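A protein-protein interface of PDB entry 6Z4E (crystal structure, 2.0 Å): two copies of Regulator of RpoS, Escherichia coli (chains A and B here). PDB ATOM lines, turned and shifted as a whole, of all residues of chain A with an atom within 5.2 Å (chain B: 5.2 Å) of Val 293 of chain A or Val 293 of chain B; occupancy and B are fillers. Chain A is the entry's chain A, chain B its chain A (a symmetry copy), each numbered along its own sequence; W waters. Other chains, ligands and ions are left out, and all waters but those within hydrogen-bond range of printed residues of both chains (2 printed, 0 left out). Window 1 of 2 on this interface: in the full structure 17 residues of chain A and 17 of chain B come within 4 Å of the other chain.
The backbone carbonyl oxygen of Gln 294 of chain A sits at hydrogen-bond distance from the backbone NH of Gln 294 of chain B (2.9 Å).
O of Ala 284 of chain A lies within hydrogen-bond range of N of Ile 295 of chain A. O of Val 293 of chain A sits at hydrogen-bond distance from N of Leu 286 of chain A. ND1 of His 291 of chain A lies within hydrogen-bond range of OE1 of Gln 314 of chain A (2.7 Å). O of Val 293 of chain B lies within hydrogen-bond range of N of Leu 286 of chain B, 2.7 Å away. The backbone carbonyl oxygen (O) of His 291 of chain B sits at hydrogen-bond distance from the side-chain amide nitrogen (ND2) of Asn 287 of chain B (3.2 Å). The side-chain amide oxygen (OE1) of Gln 314 of chain B is in hydrogen-bond range of a ring nitrogen (ND1) of His 291 of chain B, at 2.7 Å.
Of the printed residues of chain B, His 291 of chain A touches Ile 295 (3.3 Å). Printed residues of chain B within 4 Å of Gln 292 of chain A: Gln 294 and Ile 295. Of the printed residues of chain B, Val 293 of chain A touches Val 293 and Gln 294. Printed residues of chain B within 4 Å of Gln 294 of chain A: Gln 292, Val 293 and Gln 294. Printed residues of chain A within 4 Å of Gln 292 of chain B: Gln 294 and Ile 295. Of the printed residues of chain A, Val 293 of chain B touches Val 293 and Gln 294. Of the printed residues of chain A, Ile 295 of chain B touches His 291 and Gln 292. Gln 314 of chain B touches none of the printed residues of chain A. The nearest printed residue of chain B that does not touch Val 293 of chain A is Ile 295 of chain B (4.04 Å).
Gln 292 of chain A touches Gln 294 of chain B, and with the chains exchanged Gln 294 of chain A touches Gln 292 of chain B. Gln 292 of chain A touches Ile 295 of chain B, and with the chains exchanged Ile 295 of chain A touches Gln 292 of chain B. Val 293 of chain A touches its own counterpart, Val 293 of chain B. Gln 294 of chain A touches its own counterpart, Gln 294 of chain B. Of the 10 pairs that touch across the chains among the printed residues, 10 have their exchanged pair printed and touching as well.
Of the 11 printed residues of chain A, 5 touch a printed residue of chain B. Printed residues of chain A that touch a printed residue of chain B: His 291, Gln 292, Val 293, Gln 294 and Ile 295. Of the 11 printed residues of chain B, 5 touch a printed residue of chain A. Among the printed residues, 10 pairs touch across the chains.
Water W1 bridges O of Gln 292 of chain A (3.1 Å) and O of Gln 294 of chain B (3.1 Å). Water W2 bridges the backbone carbonyl oxygen (O) of Gln 292 of chain B (3.1 Å) and the backbone carbonyl oxygen (O) of Gln 294 of chain A (3.1 Å).
Among the printed residues, pairs that only touch across the chains: His 291 of chain A with Ile 295 of chain B (3.3 Å), Gln 292 of chain A with Gln 294 of chain B (3.8 Å), Gln 292 of chain A with Ile 295 of chain B (3.6 Å), Val 293 of chain A with Val 293 of chain B (3.7 Å), Val 293 of chain A with Gln 294 of chain B (3.3 Å), Gln 294 of chain A with Gln 292 of chain B (3.8 Å), Gln 294 of chain A with Val 293 of chain B (3.3 Å), Ile 295 of chain A with His 291 of chain B (3.3 Å) and Ile 295 of chain A with Gln 292 of chain B (3.6 Å).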
ATOM      1  N   ALA A 284      27.758 -25.086   1.679  1.00  0.00           N
ATOM      2  CA  ALA A 284      26.697 -25.800   0.987  1.00  0.00           C
ATOM      3  C   ALA A 284      25.760 -24.824   0.297  1.00  0.00           C
ATOM      4  O   ALA A 284      25.504 -23.722   0.791  1.00  0.00           O
ATOM      5  CB  ALA A 284      25.901 -26.690   1.948  1.00  0.00           C
ATOM      6  N   THR A 285      25.251 -25.254  -0.855  1.00  0.00           N
ATOM      7  CA  THR A 285      24.168 -24.581  -1.555  1.00  0.00           C
ATOM      8  C   THR A 285      22.992 -25.539  -1.644  1.00  0.00           C
ATOM      9  O   THR A 285      23.172 -26.717  -1.974  1.00  0.00           O
ATOM     10  CB  THR A 285      24.582 -24.133  -2.961  1.00  0.00           C
ATOM     11  OG1 THR A 285      25.014 -25.273  -3.714  1.00  0.00           O
ATOM     12  CG2 THR A 285      25.708 -23.113  -2.897  1.00  0.00           C
ATOM     13  N   LEU A 286      21.799 -25.041  -1.342  1.00  0.00           N
ATOM     14  CA  LEU A 286      20.571 -25.815  -1.436  1.00  0.00           C
ATOM     15  C   LEU A 286      19.631 -25.129  -2.415  1.00  0.00           C
ATOM     16  O   LEU A 286      19.368 -23.929  -2.290  1.00  0.00           O
ATOM     17  CB  LEU A 286      19.896 -25.955  -0.071  1.00  0.00           C
ATOM     18  CG  LEU A 286      18.515 -26.603  -0.130  1.00  0.00           C
ATOM     19  CD1 LEU A 286      18.641 -28.059  -0.562  1.00  0.00           C
ATOM     20  CD2 LEU A 286      17.816 -26.489   1.210  1.00  0.00           C
ATOM     21  N   ASN A 287      19.127 -25.889  -3.381  1.00  0.00           N
ATOM     22  CA  ASN A 287      18.209 -25.366  -4.385  1.00  0.00           C
ATOM     23  C   ASN A 287      16.953 -26.222  -4.394  1.00  0.00           C
ATOM     24  O   ASN A 287      17.036 -27.446  -4.534  1.00  0.00           O
ATOM     25  CB  ASN A 287      18.867 -25.347  -5.767  1.00  0.00           C
ATOM     26  CG  ASN A 287      18.093 -24.521  -6.773  1.00  0.00           C
ATOM     27  OD1 ASN A 287      18.416 -24.512  -7.960  1.00  0.00           O
ATOM     28  ND2 ASN A 287      17.067 -23.816  -6.304  1.00  0.00           N
ATOM     29  N   HIS A 291      13.271 -21.761  -3.857  1.00  0.00           N
ATOM     30  CA  HIS A 291      14.125 -21.285  -2.780  1.00  0.00           C
ATOM     31  C   HIS A 291      15.567 -21.683  -3.054  1.00  0.00           C
ATOM     32  O   HIS A 291      15.832 -22.785  -3.544  1.00  0.00           O
ATOM     33  CB  HIS A 291      13.656 -21.856  -1.431  1.00  0.00           C
ATOM     34  CG  HIS A 291      14.066 -21.039  -0.246  1.00  0.00           C
ATOM     35  ND1 HIS A 291      14.981 -21.484   0.685  1.00  0.00           N
ATOM     36  CD2 HIS A 291      13.684 -19.807   0.164  1.00  0.00           C
ATOM     37  CE1 HIS A 291      15.143 -20.561   1.617  1.00  0.00           C
ATOM     38  NE2 HIS A 291      14.371 -19.532   1.321  1.00  0.00           N
ATOM     39  N   GLN A 292      16.496 -20.783  -2.734  1.00  0.00           N
ATOM     40  CA  GLN A 292      17.918 -21.073  -2.845  1.00  0.00           C
ATOM     41  C   GLN A 292      18.627 -20.564  -1.600  1.00  0.00           C
ATOM     42  O   GLN A 292      18.372 -19.441  -1.157  1.00  0.00           O
ATOM     43  CB  GLN A 292      18.524 -20.435  -4.099  1.00  0.00           C
ATOM     44  CG  GLN A 292      19.907 -20.958  -4.433  1.00  0.00           C
ATOM     45  CD  GLN A 292      20.719 -19.980  -5.255  1.00  0.00           C
ATOM     46  OE1 GLN A 292      20.423 -18.785  -5.286  1.00  0.00           O
ATOM     47  NE2 GLN A 292      21.752 -20.481  -5.926  1.00  0.00           N
ATOM     48  N   VAL A 293      19.505 -21.394  -1.034  1.00  0.00           N
ATOM     49  CA  VAL A 293      20.257 -21.048   0.166  1.00  0.00           C
ATOM     50  C   VAL A 293      21.721 -21.403  -0.034  1.00  0.00           C
ATOM     51  O   VAL A 293      22.047 -22.454  -0.597  1.00  0.00           O
ATOM     52  CB  VAL A 293      19.720 -21.766   1.423  1.00  0.00           C
ATOM     53  CG1 VAL A 293      20.209 -21.063   2.681  1.00  0.00           C
ATOM     54  CG2 VAL A 293      18.212 -21.834   1.413  1.00  0.00           C
ATOM     55  N   GLN A 294      22.607 -20.527   0.433  1.00  0.00           N
ATOM     56  CA  GLN A 294      24.036 -20.813   0.486  1.00  0.00           C
ATOM     57  C   GLN A 294      24.495 -20.651   1.923  1.00  0.00           C
ATOM     58  O   GLN A 294      24.257 -19.609   2.547  1.00  0.00           O
ATOM     59  CB  GLN A 294      24.846 -19.906  -0.442  1.00  0.00           C
ATOM     60  CG  GLN A 294      26.340 -20.236  -0.441  1.00  0.00           C
ATOM     61  CD  GLN A 294      27.044 -19.826  -1.721  1.00  0.00           C
ATOM     62  OE1 GLN A 294      26.408 -19.417  -2.692  1.00  0.00           O
ATOM     63  NE2 GLN A 294      28.368 -19.932  -1.727  1.00  0.00           N
ATOM     64  N   ILE A 295      25.137 -21.685   2.452  1.00  0.00           N
ATOM     65  CA  ILE A 295      25.596 -21.718   3.832  1.00  0.00           C
ATOM     66  C   ILE A 295      27.098 -21.942   3.829  1.00  0.00           C
ATOM     67  O   ILE A 295      27.619 -22.698   3.004  1.00  0.00           O
ATOM     68  CB  ILE A 295      24.881 -22.822   4.641  1.00  0.00           C
ATOM     69  CG1 ILE A 295      23.386 -22.526   4.747  1.00  0.00           C
ATOM     70  CG2 ILE A 295      25.493 -22.978   6.025  1.00  0.00           C
ATOM     71  CD1 ILE A 295      22.547 -23.758   5.001  1.00  0.00           C
ATOM     72  N   LEU A 312      18.834 -24.893   8.959  1.00  0.00           N
ATOM     73  CA  LEU A 312      18.015 -24.533   7.814  1.00  0.00           C
ATOM     74  C   LEU A 312      16.911 -25.572   7.706  1.00  0.00           C
ATOM     75  O   LEU A 312      17.195 -26.772   7.631  1.00  0.00           O
ATOM     76  CB  LEU A 312      18.861 -24.492   6.541  1.00  0.00           C
ATOM     77  CG  LEU A 312      18.145 -24.602   5.195  1.00  0.00           C
ATOM     78  CD1 LEU A 312      17.113 -23.490   5.020  1.00  0.00           C
ATOM     79  CD2 LEU A 312      19.155 -24.585   4.066  1.00  0.00           C
ATOM     80  N   GLN A 314      13.424 -26.451   5.410  1.00  0.00           N
ATOM     81  CA  GLN A 314      12.794 -26.086   4.152  1.00  0.00           C
ATOM     82  C   GLN A 314      11.826 -27.186   3.755  1.00  0.00           C
ATOM     83  O   GLN A 314      12.156 -28.370   3.860  1.00  0.00           O
ATOM     84  CB  GLN A 314      13.851 -25.872   3.062  1.00  0.00           C
ATOM     85  CG  GLN A 314      13.308 -25.879   1.649  1.00  0.00           C
ATOM     86  CD  GLN A 314      12.699 -24.547   1.259  1.00  0.00           C
ATOM     87  OE1 GLN A 314      13.310 -23.494   1.443  1.00  0.00           O
ATOM     88  NE2 GLN A 314      11.486 -24.587   0.716  1.00  0.00           N
ATOM     89  N   ALA B 284      18.367 -12.098   1.013  1.00  0.00           N
ATOM     90  CA  ALA B 284      18.984 -11.676   2.260  1.00  0.00           C
ATOM     91  C   ALA B 284      20.301 -12.402   2.476  1.00  0.00           C
ATOM     92  O   ALA B 284      20.458 -13.569   2.105  1.00  0.00           O
ATOM     93  CB  ALA B 284      18.056 -11.921   3.455  1.00  0.00           C
ATOM     94  N   THR B 285      21.243 -11.687   3.086  1.00  0.00           N
ATOM     95  CA  THR B 285      22.483 -12.256   3.589  1.00  0.00           C
ATOM     96  C   THR B 285      22.527 -12.043   5.093  1.00  0.00           C
ATOM     97  O   THR B 285      22.226 -10.945   5.577  1.00  0.00           O
ATOM     98  CB  THR B 285      23.714 -11.619   2.937  1.00  0.00           C
ATOM     99  OG1 THR B 285      23.698 -10.206   3.170  1.00  0.00           O
ATOM    100  CG2 THR B 285      23.734 -11.885   1.440  1.00  0.00           C
ATOM    101  N   LEU B 286      22.892 -13.088   5.827  1.00  0.00           N
ATOM    102  CA  LEU B 286      23.039 -13.025   7.274  1.00  0.00           C
ATOM    103  C   LEU B 286      24.470 -13.387   7.638  1.00  0.00           C
ATOM    104  O   LEU B 286      24.982 -14.424   7.204  1.00  0.00           O
ATOM    105  CB  LEU B 286      22.063 -13.973   7.973  1.00  0.00           C
ATOM    106  CG  LEU B 286      22.288 -14.086   9.478  1.00  0.00           C
ATOM    107  CD1 LEU B 286      21.967 -12.759  10.155  1.00  0.00           C
ATOM    108  CD2 LEU B 286      21.454 -15.212  10.058  1.00  0.00           C
ATOM    109  N   ASN B 287      25.110 -12.538   8.434  1.00  0.00           N
ATOM    110  CA  ASN B 287      26.484 -12.761   8.869  1.00  0.00           C
ATOM    111  C   ASN B 287      26.534 -12.700  10.388  1.00  0.00           C
ATOM    112  O   ASN B 287      26.085 -11.716  10.983  1.00  0.00           O
ATOM    113  CB  ASN B 287      27.425 -11.726   8.250  1.00  0.00           C
ATOM    114  CG  ASN B 287      28.886 -12.100   8.397  1.00  0.00           C
ATOM    115  OD1 ASN B 287      29.773 -11.311   8.071  1.00  0.00           O
ATOM    116  ND2 ASN B 287      29.145 -13.309   8.886  1.00  0.00           N
ATOM    117  N   HIS B 291      29.272 -17.782  11.029  1.00  0.00           N
ATOM    118  CA  HIS B 291      28.299 -18.337  10.102  1.00  0.00           C
ATOM    119  C   HIS B 291      27.871 -17.271   9.107  1.00  0.00           C
ATOM    120  O   HIS B 291      27.708 -16.102   9.470  1.00  0.00           O
ATOM    121  CB  HIS B 291      27.079 -18.879  10.866  1.00  0.00           C
ATOM    122  CG  HIS B 291      26.311 -19.931  10.127  1.00  0.00           C
ATOM    123  ND1 HIS B 291      25.036 -19.725   9.649  1.00  0.00           N
ATOM    124  CD2 HIS B 291      26.639 -21.199   9.786  1.00  0.00           C
ATOM    125  CE1 HIS B 291      24.609 -20.821   9.047  1.00  0.00           C
ATOM    126  NE2 HIS B 291      25.565 -21.729   9.112  1.00  0.00           N
ATOM    127  N   GLN B 292      27.691 -17.677   7.851  1.00  0.00           N
ATOM    128  CA  GLN B 292      27.183 -16.785   6.818  1.00  0.00           C
ATOM    129  C   GLN B 292      26.131 -17.520   6.002  1.00  0.00           C
ATOM    130  O   GLN B 292      26.340 -18.673   5.617  1.00  0.00           O
ATOM    131  CB  GLN B 292      28.306 -16.284   5.908  1.00  0.00           C
ATOM    132  CG  GLN B 292      27.895 -15.120   5.027  1.00  0.00           C
ATOM    133  CD  GLN B 292      28.740 -15.007   3.776  1.00  0.00           C
ATOM    134  OE1 GLN B 292      29.389 -15.968   3.365  1.00  0.00           O
ATOM    135  NE2 GLN B 292      28.735 -13.828   3.161  1.00  0.00           N
ATOM    136  N   VAL B 293      25.002 -16.855   5.751  1.00  0.00           N
ATOM    137  CA  VAL B 293      23.902 -17.430   4.985  1.00  0.00           C
ATOM    138  C   VAL B 293      23.425 -16.425   3.950  1.00  0.00           C
ATOM    139  O   VAL B 293      23.324 -15.226   4.232  1.00  0.00           O
ATOM    140  CB  VAL B 293      22.717 -17.847   5.883  1.00  0.00           C
ATOM    141  CG1 VAL B 293      21.814 -18.823   5.142  1.00  0.00           C
ATOM    142  CG2 VAL B 293      23.198 -18.456   7.178  1.00  0.00           C
ATOM    143  N   GLN B 294      23.126 -16.914   2.750  1.00  0.00           N
ATOM    144  CA  GLN B 294      22.480 -16.113   1.717  1.00  0.00           C
ATOM    145  C   GLN B 294      21.199 -16.817   1.308  1.00  0.00           C
ATOM    146  O   GLN B 294      21.216 -18.004   0.961  1.00  0.00           O
ATOM    147  CB  GLN B 294      23.382 -15.892   0.503  1.00  0.00           C
ATOM    148  CG  GLN B 294      22.739 -15.001  -0.562  1.00  0.00           C
ATOM    149  CD  GLN B 294      23.752 -14.279  -1.431  1.00  0.00           C
ATOM    150  OE1 GLN B 294      24.954 -14.316  -1.167  1.00  0.00           O
ATOM    151  NE2 GLN B 294      23.269 -13.619  -2.477  1.00  0.00           N
ATOM    152  N   ILE B 295      20.090 -16.090   1.364  1.00  0.00           N
ATOM    153  CA  ILE B 295      18.771 -16.623   1.059  1.00  0.00           C
ATOM    154  C   ILE B 295      18.174 -15.803  -0.070  1.00  0.00           C
ATOM    155  O   ILE B 295      18.358 -14.583  -0.126  1.00  0.00           O
ATOM    156  CB  ILE B 295      17.849 -16.598   2.298  1.00  0.00           C
ATOM    157  CG1 ILE B 295      18.389 -17.524   3.387  1.00  0.00           C
ATOM    158  CG2 ILE B 295      16.422 -16.979   1.934  1.00  0.00           C
ATOM    159  CD1 ILE B 295      17.914 -17.157   4.776  1.00  0.00           C
ATOM    160  N   LEU B 312      15.351 -20.158   8.669  1.00  0.00           N
ATOM    161  CA  LEU B 312      16.738 -20.144   9.105  1.00  0.00           C
ATOM    162  C   LEU B 312      16.739 -19.832  10.592  1.00  0.00           C
ATOM    163  O   LEU B 312      16.180 -18.812  11.012  1.00  0.00           O
ATOM    164  CB  LEU B 312      17.536 -19.102   8.321  1.00  0.00           C
ATOM    165  CG  LEU B 312      18.849 -18.599   8.921  1.00  0.00           C
ATOM    166  CD1 LEU B 312      19.827 -19.745   9.162  1.00  0.00           C
ATOM    167  CD2 LEU B 312      19.462 -17.546   8.019  1.00  0.00           C
ATOM    168  N   GLN B 314      19.430 -19.477  13.884  1.00  0.00           N
ATOM    169  CA  GLN B 314      20.849 -19.322  14.154  1.00  0.00           C
ATOM    170  C   GLN B 314      21.020 -18.747  15.550  1.00  0.00           C
ATOM    171  O   GLN B 314      20.302 -17.819  15.929  1.00  0.00           O
ATOM    172  CB  GLN B 314      21.501 -18.410  13.107  1.00  0.00           C
ATOM    173  CG  GLN B 314      22.857 -17.867  13.502  1.00  0.00           C
ATOM    174  CD  GLN B 314      23.971 -18.866  13.262  1.00  0.00           C
ATOM    175  OE1 GLN B 314      24.076 -19.447  12.182  1.00  0.00           O
ATOM    176  NE2 GLN B 314      24.810 -19.073  14.271  1.00  0.00           N
HETATM  177  O   HOH W   1      20.974 -18.085  -2.126  1.00  0.00           O
HETATM  178  O   HOH W   2      26.878 -17.961   2.659  1.00  0.00           O
